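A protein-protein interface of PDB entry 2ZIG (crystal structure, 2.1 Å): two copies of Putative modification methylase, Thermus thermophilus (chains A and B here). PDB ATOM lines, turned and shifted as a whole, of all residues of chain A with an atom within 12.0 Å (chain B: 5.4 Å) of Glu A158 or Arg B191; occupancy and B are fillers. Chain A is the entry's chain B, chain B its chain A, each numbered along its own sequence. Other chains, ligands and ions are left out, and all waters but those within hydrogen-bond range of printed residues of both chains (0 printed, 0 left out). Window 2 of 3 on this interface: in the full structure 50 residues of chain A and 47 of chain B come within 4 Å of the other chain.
The guanidinium group (NE) of Arg B187 lies within salt-bridge range of the side-chain carboxylate (OE1) of Glu A158 (2.8 Å).
The guanidinium group (NH2) of Arg B191 lies within salt-bridge range of the side-chain carboxylate (OE2) of Glu A158 (3.4 Å).
N of Gly A160 sits at hydrogen-bond distance from O of Met B231 (2.8 Å).
N of Leu B192 is in hydrogen-bond range of O of Tyr A157 (2.8 Å).
The guanidinium group (NH1) of Arg B191 sits close to the backbone carbonyl oxygen (O) of Arg B187, at 3.3 Å.
OG of Ser B190 is in hydrogen-bond range of O of Gln B186 (2.7 Å).
Tyr A157 touches Arg B191 (O to CA, 3.5 Å).
Phe B197 touches Tyr A157.
Phe B197 touches Glu A158.
Ser B190 touches Pro A159.
Arg B230 touches Pro A159.
O of Met B231 touches CA of Pro A159, 3.1 Å away.
Pro A159 touches Phe B234 (CD to CE1, 3.7 Å).
Phe B197 touches Ala A161 (CZ to CB, 3.7 Å).
O of Ala A161 touches CE2 of Phe B201, at 3.3 Å.
CG1 of Ile A163 touches CA of Phe B201, 3.9 Å away.
Printed residues of chain B within 4 Å of Tyr A157: Arg B191 (3.5 Å), Leu B192 (2.8 Å) and Phe B197 (3.3 Å).
Glu A158 touches just these residues of chain B: Arg B187, Arg B191 and Phe B197.
Printed residues of chain B within 4 Å of Pro A159: Ser B190 (3.7 Å), Arg B230 (3.4 Å), Met B231 (3.1 Å) and Phe B234 (3.7 Å).
Of the printed residues of chain B, Ile A163 touches Phe B201.
Gln B184 touches none of the printed residues of chain A.
Of chain A, only Glu A158 (2.8 Å) comes within 4 Å of Arg B187.
Glu B188 touches none of the printed residues of chain A.
Ser B190 touches one residue of chain A.
Arg B191 touches just these residues of chain A: Tyr A157 (3.5 Å) and Glu A158 (3.4 Å).
Of the printed residues of chain A, Leu B192 touches Tyr A157 (2.8 Å).
No residue of chain A comes within 4 Å of Pro B193.
Of the printed residues of chain A, Met B231 touches Pro A159 (3.1 Å) and Gly A160 (2.8 Å).
Of the printed residues of chain A, Phe B234 touches Pro A159 (3.7 Å).
The nearest residue of chain B that does not touch Glu A158 is Phe B201 (4.1 Å).
The nearest printed residue of chain A that does not touch Phe B234 is Glu A158 (4.5 Å).
Of the 8 printed residues of chain A, 6 touch a printed residue of chain B.
Printed residues of chain A that touch a printed residue of chain B: Tyr A157, Glu A158, Pro A159, Gly A160, Ala A161 and Ile A163.
Printed residues of chain B that touch a printed residue of chain A: Arg B187, Ser B190, Arg B191, Leu B192, Phe B197, Phe B201, Arg B230, Met B231 and Phe B234.
Hydrophobic or aromatic side chains of chain B that line the printed part of chain A: Leu B192, Phe B197, Phe B201 and Phe B234.
No position is printed for both chains.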
ATOM      1  N   PRO A 156      33.499   0.516 -23.240  1.00  0.00           N
ATOM      2  CA  PRO A 156      33.386   0.040 -21.854  1.00  0.00           C
ATOM      3  C   PRO A 156      31.947   0.033 -21.332  1.00  0.00           C
ATOM      4  O   PRO A 156      31.250  -0.976 -21.426  1.00  0.00           O
ATOM      5  CB  PRO A 156      34.279   1.010 -21.087  1.00  0.00           C
ATOM      6  CG  PRO A 156      34.117   2.296 -21.873  1.00  0.00           C
ATOM      7  CD  PRO A 156      34.208   1.809 -23.302  1.00  0.00           C
ATOM      8  N   TYR A 157      31.508   1.163 -20.789  1.00  0.00           N
ATOM      9  CA  TYR A 157      30.157   1.288 -20.243  1.00  0.00           C
ATOM     10  C   TYR A 157      29.950   0.414 -19.009  1.00  0.00           C
ATOM     11  O   TYR A 157      28.847  -0.057 -18.746  1.00  0.00           O
ATOM     12  CB  TYR A 157      29.112   0.945 -21.314  1.00  0.00           C
ATOM     13  CG  TYR A 157      29.078   1.939 -22.457  1.00  0.00           C
ATOM     14  CD1 TYR A 157      29.027   3.310 -22.209  1.00  0.00           C
ATOM     15  CD2 TYR A 157      29.116   1.515 -23.786  1.00  0.00           C
ATOM     16  CE1 TYR A 157      29.018   4.234 -23.249  1.00  0.00           C
ATOM     17  CE2 TYR A 157      29.107   2.436 -24.834  1.00  0.00           C
ATOM     18  CZ  TYR A 157      29.060   3.791 -24.557  1.00  0.00           C
ATOM     19  OH  TYR A 157      29.057   4.710 -25.583  1.00  0.00           O
ATOM     20  N   GLU A 158      31.018   0.221 -18.247  1.00  0.00           N
ATOM     21  CA  GLU A 158      30.967  -0.594 -17.039  1.00  0.00           C
ATOM     22  C   GLU A 158      31.207   0.264 -15.810  1.00  0.00           C
ATOM     23  O   GLU A 158      31.661   1.397 -15.922  1.00  0.00           O
ATOM     24  CB  GLU A 158      32.013  -1.706 -17.115  1.00  0.00           C
ATOM     25  CG  GLU A 158      31.646  -2.800 -18.103  1.00  0.00           C
ATOM     26  CD  GLU A 158      32.714  -3.866 -18.247  1.00  0.00           C
ATOM     27  OE1 GLU A 158      33.204  -4.370 -17.216  1.00  0.00           O
ATOM     28  OE2 GLU A 158      33.055  -4.210 -19.397  1.00  0.00           O
ATOM     29  N   PRO A 159      30.904  -0.267 -14.616  1.00  0.00           N
ATOM     30  CA  PRO A 159      31.096   0.475 -13.366  1.00  0.00           C
ATOM     31  C   PRO A 159      32.538   0.913 -13.114  1.00  0.00           C
ATOM     32  O   PRO A 159      33.471   0.382 -13.710  1.00  0.00           O
ATOM     33  CB  PRO A 159      30.614  -0.513 -12.308  1.00  0.00           C
ATOM     34  CG  PRO A 159      29.546  -1.279 -13.027  1.00  0.00           C
ATOM     35  CD  PRO A 159      30.209  -1.541 -14.361  1.00  0.00           C
ATOM     36  N   GLY A 160      32.706   1.896 -12.231  1.00  0.00           N
ATOM     37  CA  GLY A 160      34.036   2.366 -11.881  1.00  0.00           C
ATOM     38  C   GLY A 160      34.712   3.351 -12.814  1.00  0.00           C
ATOM     39  O   GLY A 160      35.881   3.677 -12.614  1.00  0.00           O
ATOM     40  N   ALA A 161      34.004   3.825 -13.833  1.00  0.00           N
ATOM     41  CA  ALA A 161      34.597   4.776 -14.763  1.00  0.00           C
ATOM     42  C   ALA A 161      34.901   6.078 -14.049  1.00  0.00           C
ATOM     43  O   ALA A 161      34.213   6.453 -13.103  1.00  0.00           O
ATOM     44  CB  ALA A 161      33.654   5.031 -15.928  1.00  0.00           C
ATOM     45  N   ILE A 162      35.937   6.769 -14.506  1.00  0.00           N
ATOM     46  CA  ILE A 162      36.330   8.034 -13.905  1.00  0.00           C
ATOM     47  C   ILE A 162      35.482   9.149 -14.486  1.00  0.00           C
ATOM     48  O   ILE A 162      35.213   9.156 -15.685  1.00  0.00           O
ATOM     49  CB  ILE A 162      37.808   8.359 -14.192  1.00  0.00           C
ATOM     50  CG1 ILE A 162      38.711   7.420 -13.397  1.00  0.00           C
ATOM     51  CG2 ILE A 162      38.107   9.804 -13.823  1.00  0.00           C
ATOM     52  CD1 ILE A 162      40.191   7.561 -13.729  1.00  0.00           C
ATOM     53  N   ILE A 163      35.055  10.081 -13.640  1.00  0.00           N
ATOM     54  CA  ILE A 163      34.265  11.211 -14.107  1.00  0.00           C
ATOM     55  C   ILE A 163      35.181  12.413 -14.317  1.00  0.00           C
ATOM     56  O   ILE A 163      35.862  12.869 -13.392  1.00  0.00           O
ATOM     57  CB  ILE A 163      33.152  11.580 -13.116  1.00  0.00           C
ATOM     58  CG1 ILE A 163      32.114  10.455 -13.063  1.00  0.00           C
ATOM     59  CG2 ILE A 163      32.482  12.881 -13.560  1.00  0.00           C
ATOM     60  CD1 ILE A 163      31.048  10.638 -12.011  1.00  0.00           C
ATOM     61  N   GLN B 184      33.434 -12.440 -15.684  1.00  0.00           N
ATOM     62  CA  GLN B 184      32.873 -12.031 -16.961  1.00  0.00           C
ATOM     63  C   GLN B 184      31.367 -11.855 -16.867  1.00  0.00           C
ATOM     64  O   GLN B 184      30.803 -10.938 -17.467  1.00  0.00           O
ATOM     65  CB  GLN B 184      33.215 -13.054 -18.035  1.00  0.00           C
ATOM     66  CG  GLN B 184      34.660 -13.002 -18.462  1.00  0.00           C
ATOM     67  CD  GLN B 184      34.997 -14.083 -19.460  1.00  0.00           C
ATOM     68  OE1 GLN B 184      34.946 -15.273 -19.142  1.00  0.00           O
ATOM     69  NE2 GLN B 184      35.346 -13.678 -20.676  1.00  0.00           N
ATOM     70  N   GLN B 186      29.609 -11.045 -14.142  1.00  0.00           N
ATOM     71  CA  GLN B 186      29.336  -9.837 -13.360  1.00  0.00           C
ATOM     72  C   GLN B 186      29.459  -8.609 -14.253  1.00  0.00           C
ATOM     73  O   GLN B 186      28.594  -7.738 -14.263  1.00  0.00           O
ATOM     74  CB  GLN B 186      30.335  -9.686 -12.208  1.00  0.00           C
ATOM     75  CG  GLN B 186      30.160 -10.648 -11.041  1.00  0.00           C
ATOM     76  CD  GLN B 186      31.116 -10.316  -9.905  1.00  0.00           C
ATOM     77  OE1 GLN B 186      32.333 -10.363 -10.078  1.00  0.00           O
ATOM     78  NE2 GLN B 186      30.568  -9.956  -8.741  1.00  0.00           N
ATOM     79  N   ARG B 187      30.554  -8.544 -14.994  1.00  0.00           N
ATOM     80  CA  ARG B 187      30.786  -7.426 -15.881  1.00  0.00           C
ATOM     81  C   ARG B 187      29.662  -7.288 -16.886  1.00  0.00           C
ATOM     82  O   ARG B 187      29.189  -6.184 -17.135  1.00  0.00           O
ATOM     83  CB  ARG B 187      32.101  -7.600 -16.626  1.00  0.00           C
ATOM     84  CG  ARG B 187      33.336  -7.446 -15.772  1.00  0.00           C
ATOM     85  CD  ARG B 187      34.572  -7.665 -16.623  1.00  0.00           C
ATOM     86  NE  ARG B 187      34.623  -6.742 -17.750  1.00  0.00           N
ATOM     87  CZ  ARG B 187      35.302  -6.968 -18.870  1.00  0.00           C
ATOM     88  NH1 ARG B 187      35.989  -8.095 -19.016  1.00  0.00           N
ATOM     89  NH2 ARG B 187      35.301  -6.065 -19.846  1.00  0.00           N
ATOM     90  N   GLU B 188      29.235  -8.408 -17.467  1.00  0.00           N
ATOM     91  CA  GLU B 188      28.163  -8.381 -18.460  1.00  0.00           C
ATOM     92  C   GLU B 188      26.816  -7.951 -17.900  1.00  0.00           C
ATOM     93  O   GLU B 188      26.120  -7.163 -18.522  1.00  0.00           O
ATOM     94  CB  GLU B 188      28.030  -9.748 -19.141  1.00  0.00           C
ATOM     95  CG  GLU B 188      29.052  -9.966 -20.243  1.00  0.00           C
ATOM     96  CD  GLU B 188      29.409 -11.426 -20.425  1.00  0.00           C
ATOM     97  OE1 GLU B 188      28.505 -12.278 -20.279  1.00  0.00           O
ATOM     98  OE2 GLU B 188      30.593 -11.715 -20.721  1.00  0.00           O
ATOM     99  N   LYS B 189      26.452  -8.463 -16.728  1.00  0.00           N
ATOM    100  CA  LYS B 189      25.181  -8.110 -16.112  1.00  0.00           C
ATOM    101  C   LYS B 189      25.240  -6.783 -15.361  1.00  0.00           C
ATOM    102  O   LYS B 189      24.269  -6.379 -14.733  1.00  0.00           O
ATOM    103  CB  LYS B 189      24.738  -9.209 -15.153  1.00  0.00           C
ATOM    104  CG  LYS B 189      24.356 -10.502 -15.840  1.00  0.00           C
ATOM    105  CD  LYS B 189      23.893 -11.534 -14.830  1.00  0.00           C
ATOM    106  CE  LYS B 189      23.513 -12.839 -15.504  1.00  0.00           C
ATOM    107  NZ  LYS B 189      23.354 -13.936 -14.498  1.00  0.00           N
ATOM    108  N   SER B 190      26.378  -6.106 -15.429  1.00  0.00           N
ATOM    109  CA  SER B 190      26.537  -4.828 -14.749  1.00  0.00           C
ATOM    110  C   SER B 190      26.781  -3.723 -15.753  1.00  0.00           C
ATOM    111  O   SER B 190      26.846  -2.557 -15.383  1.00  0.00           O
ATOM    112  CB  SER B 190      27.706  -4.882 -13.758  1.00  0.00           C
ATOM    113  OG  SER B 190      27.476  -5.844 -12.740  1.00  0.00           O
ATOM    114  N   ARG B 191      26.947  -4.087 -17.023  1.00  0.00           N
ATOM    115  CA  ARG B 191      27.168  -3.085 -18.055  1.00  0.00           C
ATOM    116  C   ARG B 191      25.970  -2.147 -18.070  1.00  0.00           C
ATOM    117  O   ARG B 191      24.845  -2.558 -17.794  1.00  0.00           O
ATOM    118  CB  ARG B 191      27.312  -3.730 -19.438  1.00  0.00           C
ATOM    119  CG  ARG B 191      28.675  -4.331 -19.727  1.00  0.00           C
ATOM    120  CD  ARG B 191      28.767  -4.791 -21.189  1.00  0.00           C
ATOM    121  NE  ARG B 191      30.112  -5.227 -21.565  1.00  0.00           N
ATOM    122  CZ  ARG B 191      30.726  -6.299 -21.072  1.00  0.00           C
ATOM    123  NH1 ARG B 191      30.122  -7.062 -20.173  1.00  0.00           N
ATOM    124  NH2 ARG B 191      31.948  -6.608 -21.481  1.00  0.00           N
ATOM    125  N   LEU B 192      26.204  -0.884 -18.392  1.00  0.00           N
ATOM    126  CA  LEU B 192      25.107   0.077 -18.439  1.00  0.00           C
ATOM    127  C   LEU B 192      24.753   0.427 -19.880  1.00  0.00           C
ATOM    128  O   LEU B 192      25.633   0.548 -20.725  1.00  0.00           O
ATOM    129  CB  LEU B 192      25.500   1.367 -17.714  1.00  0.00           C
ATOM    130  CG  LEU B 192      25.784   1.290 -16.215  1.00  0.00           C
ATOM    131  CD1 LEU B 192      26.081   2.677 -15.698  1.00  0.00           C
ATOM    132  CD2 LEU B 192      24.584   0.708 -15.489  1.00  0.00           C
ATOM    133  N   PRO B 193      23.456   0.575 -20.179  1.00  0.00           N
ATOM    134  CA  PRO B 193      23.091   0.932 -21.555  1.00  0.00           C
ATOM    135  C   PRO B 193      23.764   2.278 -21.821  1.00  0.00           C
ATOM    136  O   PRO B 193      23.886   3.101 -20.907  1.00  0.00           O
ATOM    137  CB  PRO B 193      21.575   1.050 -21.494  1.00  0.00           C
ATOM    138  CG  PRO B 193      21.208   0.060 -20.436  1.00  0.00           C
ATOM    139  CD  PRO B 193      22.258   0.288 -19.371  1.00  0.00           C
ATOM    140  N   PHE B 197      24.816   5.301 -19.073  1.00  0.00           N
ATOM    141  CA  PHE B 197      26.202   5.593 -18.774  1.00  0.00           C
ATOM    142  C   PHE B 197      26.484   7.082 -18.888  1.00  0.00           C
ATOM    143  O   PHE B 197      27.021   7.692 -17.964  1.00  0.00           O
ATOM    144  CB  PHE B 197      27.129   4.836 -19.728  1.00  0.00           C
ATOM    145  CG  PHE B 197      28.593   5.012 -19.419  1.00  0.00           C
ATOM    146  CD1 PHE B 197      29.217   4.218 -18.463  1.00  0.00           C
ATOM    147  CD2 PHE B 197      29.336   6.000 -20.058  1.00  0.00           C
ATOM    148  CE1 PHE B 197      30.559   4.405 -18.142  1.00  0.00           C
ATOM    149  CE2 PHE B 197      30.681   6.199 -19.744  1.00  0.00           C
ATOM    150  CZ  PHE B 197      31.294   5.398 -18.781  1.00  0.00           C
ATOM    151  N   PHE B 201      27.683   9.103 -15.419  1.00  0.00           N
ATOM    152  CA  PHE B 201      29.043   9.570 -15.251  1.00  0.00           C
ATOM    153  C   PHE B 201      29.274  11.000 -15.739  1.00  0.00           C
ATOM    154  O   PHE B 201      29.883  11.240 -16.780  1.00  0.00           O
ATOM    155  CB  PHE B 201      30.022   8.599 -15.924  1.00  0.00           C
ATOM    156  CG  PHE B 201      30.057   7.238 -15.284  1.00  0.00           C
ATOM    157  CD1 PHE B 201      29.123   6.267 -15.625  1.00  0.00           C
ATOM    158  CD2 PHE B 201      31.009   6.936 -14.317  1.00  0.00           C
ATOM    159  CE1 PHE B 201      29.134   5.007 -15.011  1.00  0.00           C
ATOM    160  CE2 PHE B 201      31.028   5.684 -13.696  1.00  0.00           C
ATOM    161  CZ  PHE B 201      30.089   4.719 -14.046  1.00  0.00           C
ATOM    162  N   ARG B 230      24.648   1.145  -9.301  1.00  0.00           N
ATOM    163  CA  ARG B 230      24.942   0.697 -10.657  1.00  0.00           C
ATOM    164  C   ARG B 230      26.268   1.231 -11.195  1.00  0.00           C
ATOM    165  O   ARG B 230      26.890   0.614 -12.045  1.00  0.00           O
ATOM    166  CB  ARG B 230      23.801   1.105 -11.590  1.00  0.00           C
ATOM    167  CG  ARG B 230      22.445   0.519 -11.198  1.00  0.00           C
ATOM    168  CD  ARG B 230      21.342   1.003 -12.142  1.00  0.00           C
ATOM    169  NE  ARG B 230      21.550   0.538 -13.507  1.00  0.00           N
ATOM    170  CZ  ARG B 230      21.008   1.091 -14.592  1.00  0.00           C
ATOM    171  NH1 ARG B 230      20.214   2.148 -14.487  1.00  0.00           N
ATOM    172  NH2 ARG B 230      21.261   0.580 -15.791  1.00  0.00           N
ATOM    173  N   MET B 231      26.701   2.374 -10.685  1.00  0.00           N
ATOM    174  CA  MET B 231      27.941   2.993 -11.133  1.00  0.00           C
ATOM    175  C   MET B 231      29.199   2.486 -10.457  1.00  0.00           C
ATOM    176  O   MET B 231      30.257   2.416 -11.079  1.00  0.00           O
ATOM    177  CB  MET B 231      27.890   4.506 -10.900  1.00  0.00           C
ATOM    178  CG  MET B 231      26.944   5.267 -11.786  1.00  0.00           C
ATOM    179  SD  MET B 231      26.737   6.941 -11.169  1.00  0.00           S
ATOM    180  CE  MET B 231      28.230   7.691 -11.704  1.00  0.00           C
ATOM    181  N   PHE B 234      29.240  -4.170  -8.746  1.00  0.00           N
ATOM    182  CA  PHE B 234      28.783  -5.149  -9.730  1.00  0.00           C
ATOM    183  C   PHE B 234      27.762  -6.042  -9.061  1.00  0.00           C
ATOM    184  O   PHE B 234      27.744  -6.139  -7.835  1.00  0.00           O
ATOM    185  CB  PHE B 234      29.951  -6.027 -10.186  1.00  0.00           C
ATOM    186  CG  PHE B 234      31.042  -5.278 -10.888  1.00  0.00           C
ATOM    187  CD1 PHE B 234      31.005  -5.108 -12.267  1.00  0.00           C
ATOM    188  CD2 PHE B 234      32.107  -4.740 -10.170  1.00  0.00           C
ATOM    189  CE1 PHE B 234      32.012  -4.412 -12.927  1.00  0.00           C
ATOM    190  CE2 PHE B 234      33.123  -4.042 -10.819  1.00  0.00           C
ATOM    191  CZ  PHE B 234      33.074  -3.878 -12.204  1.00  0.00           C
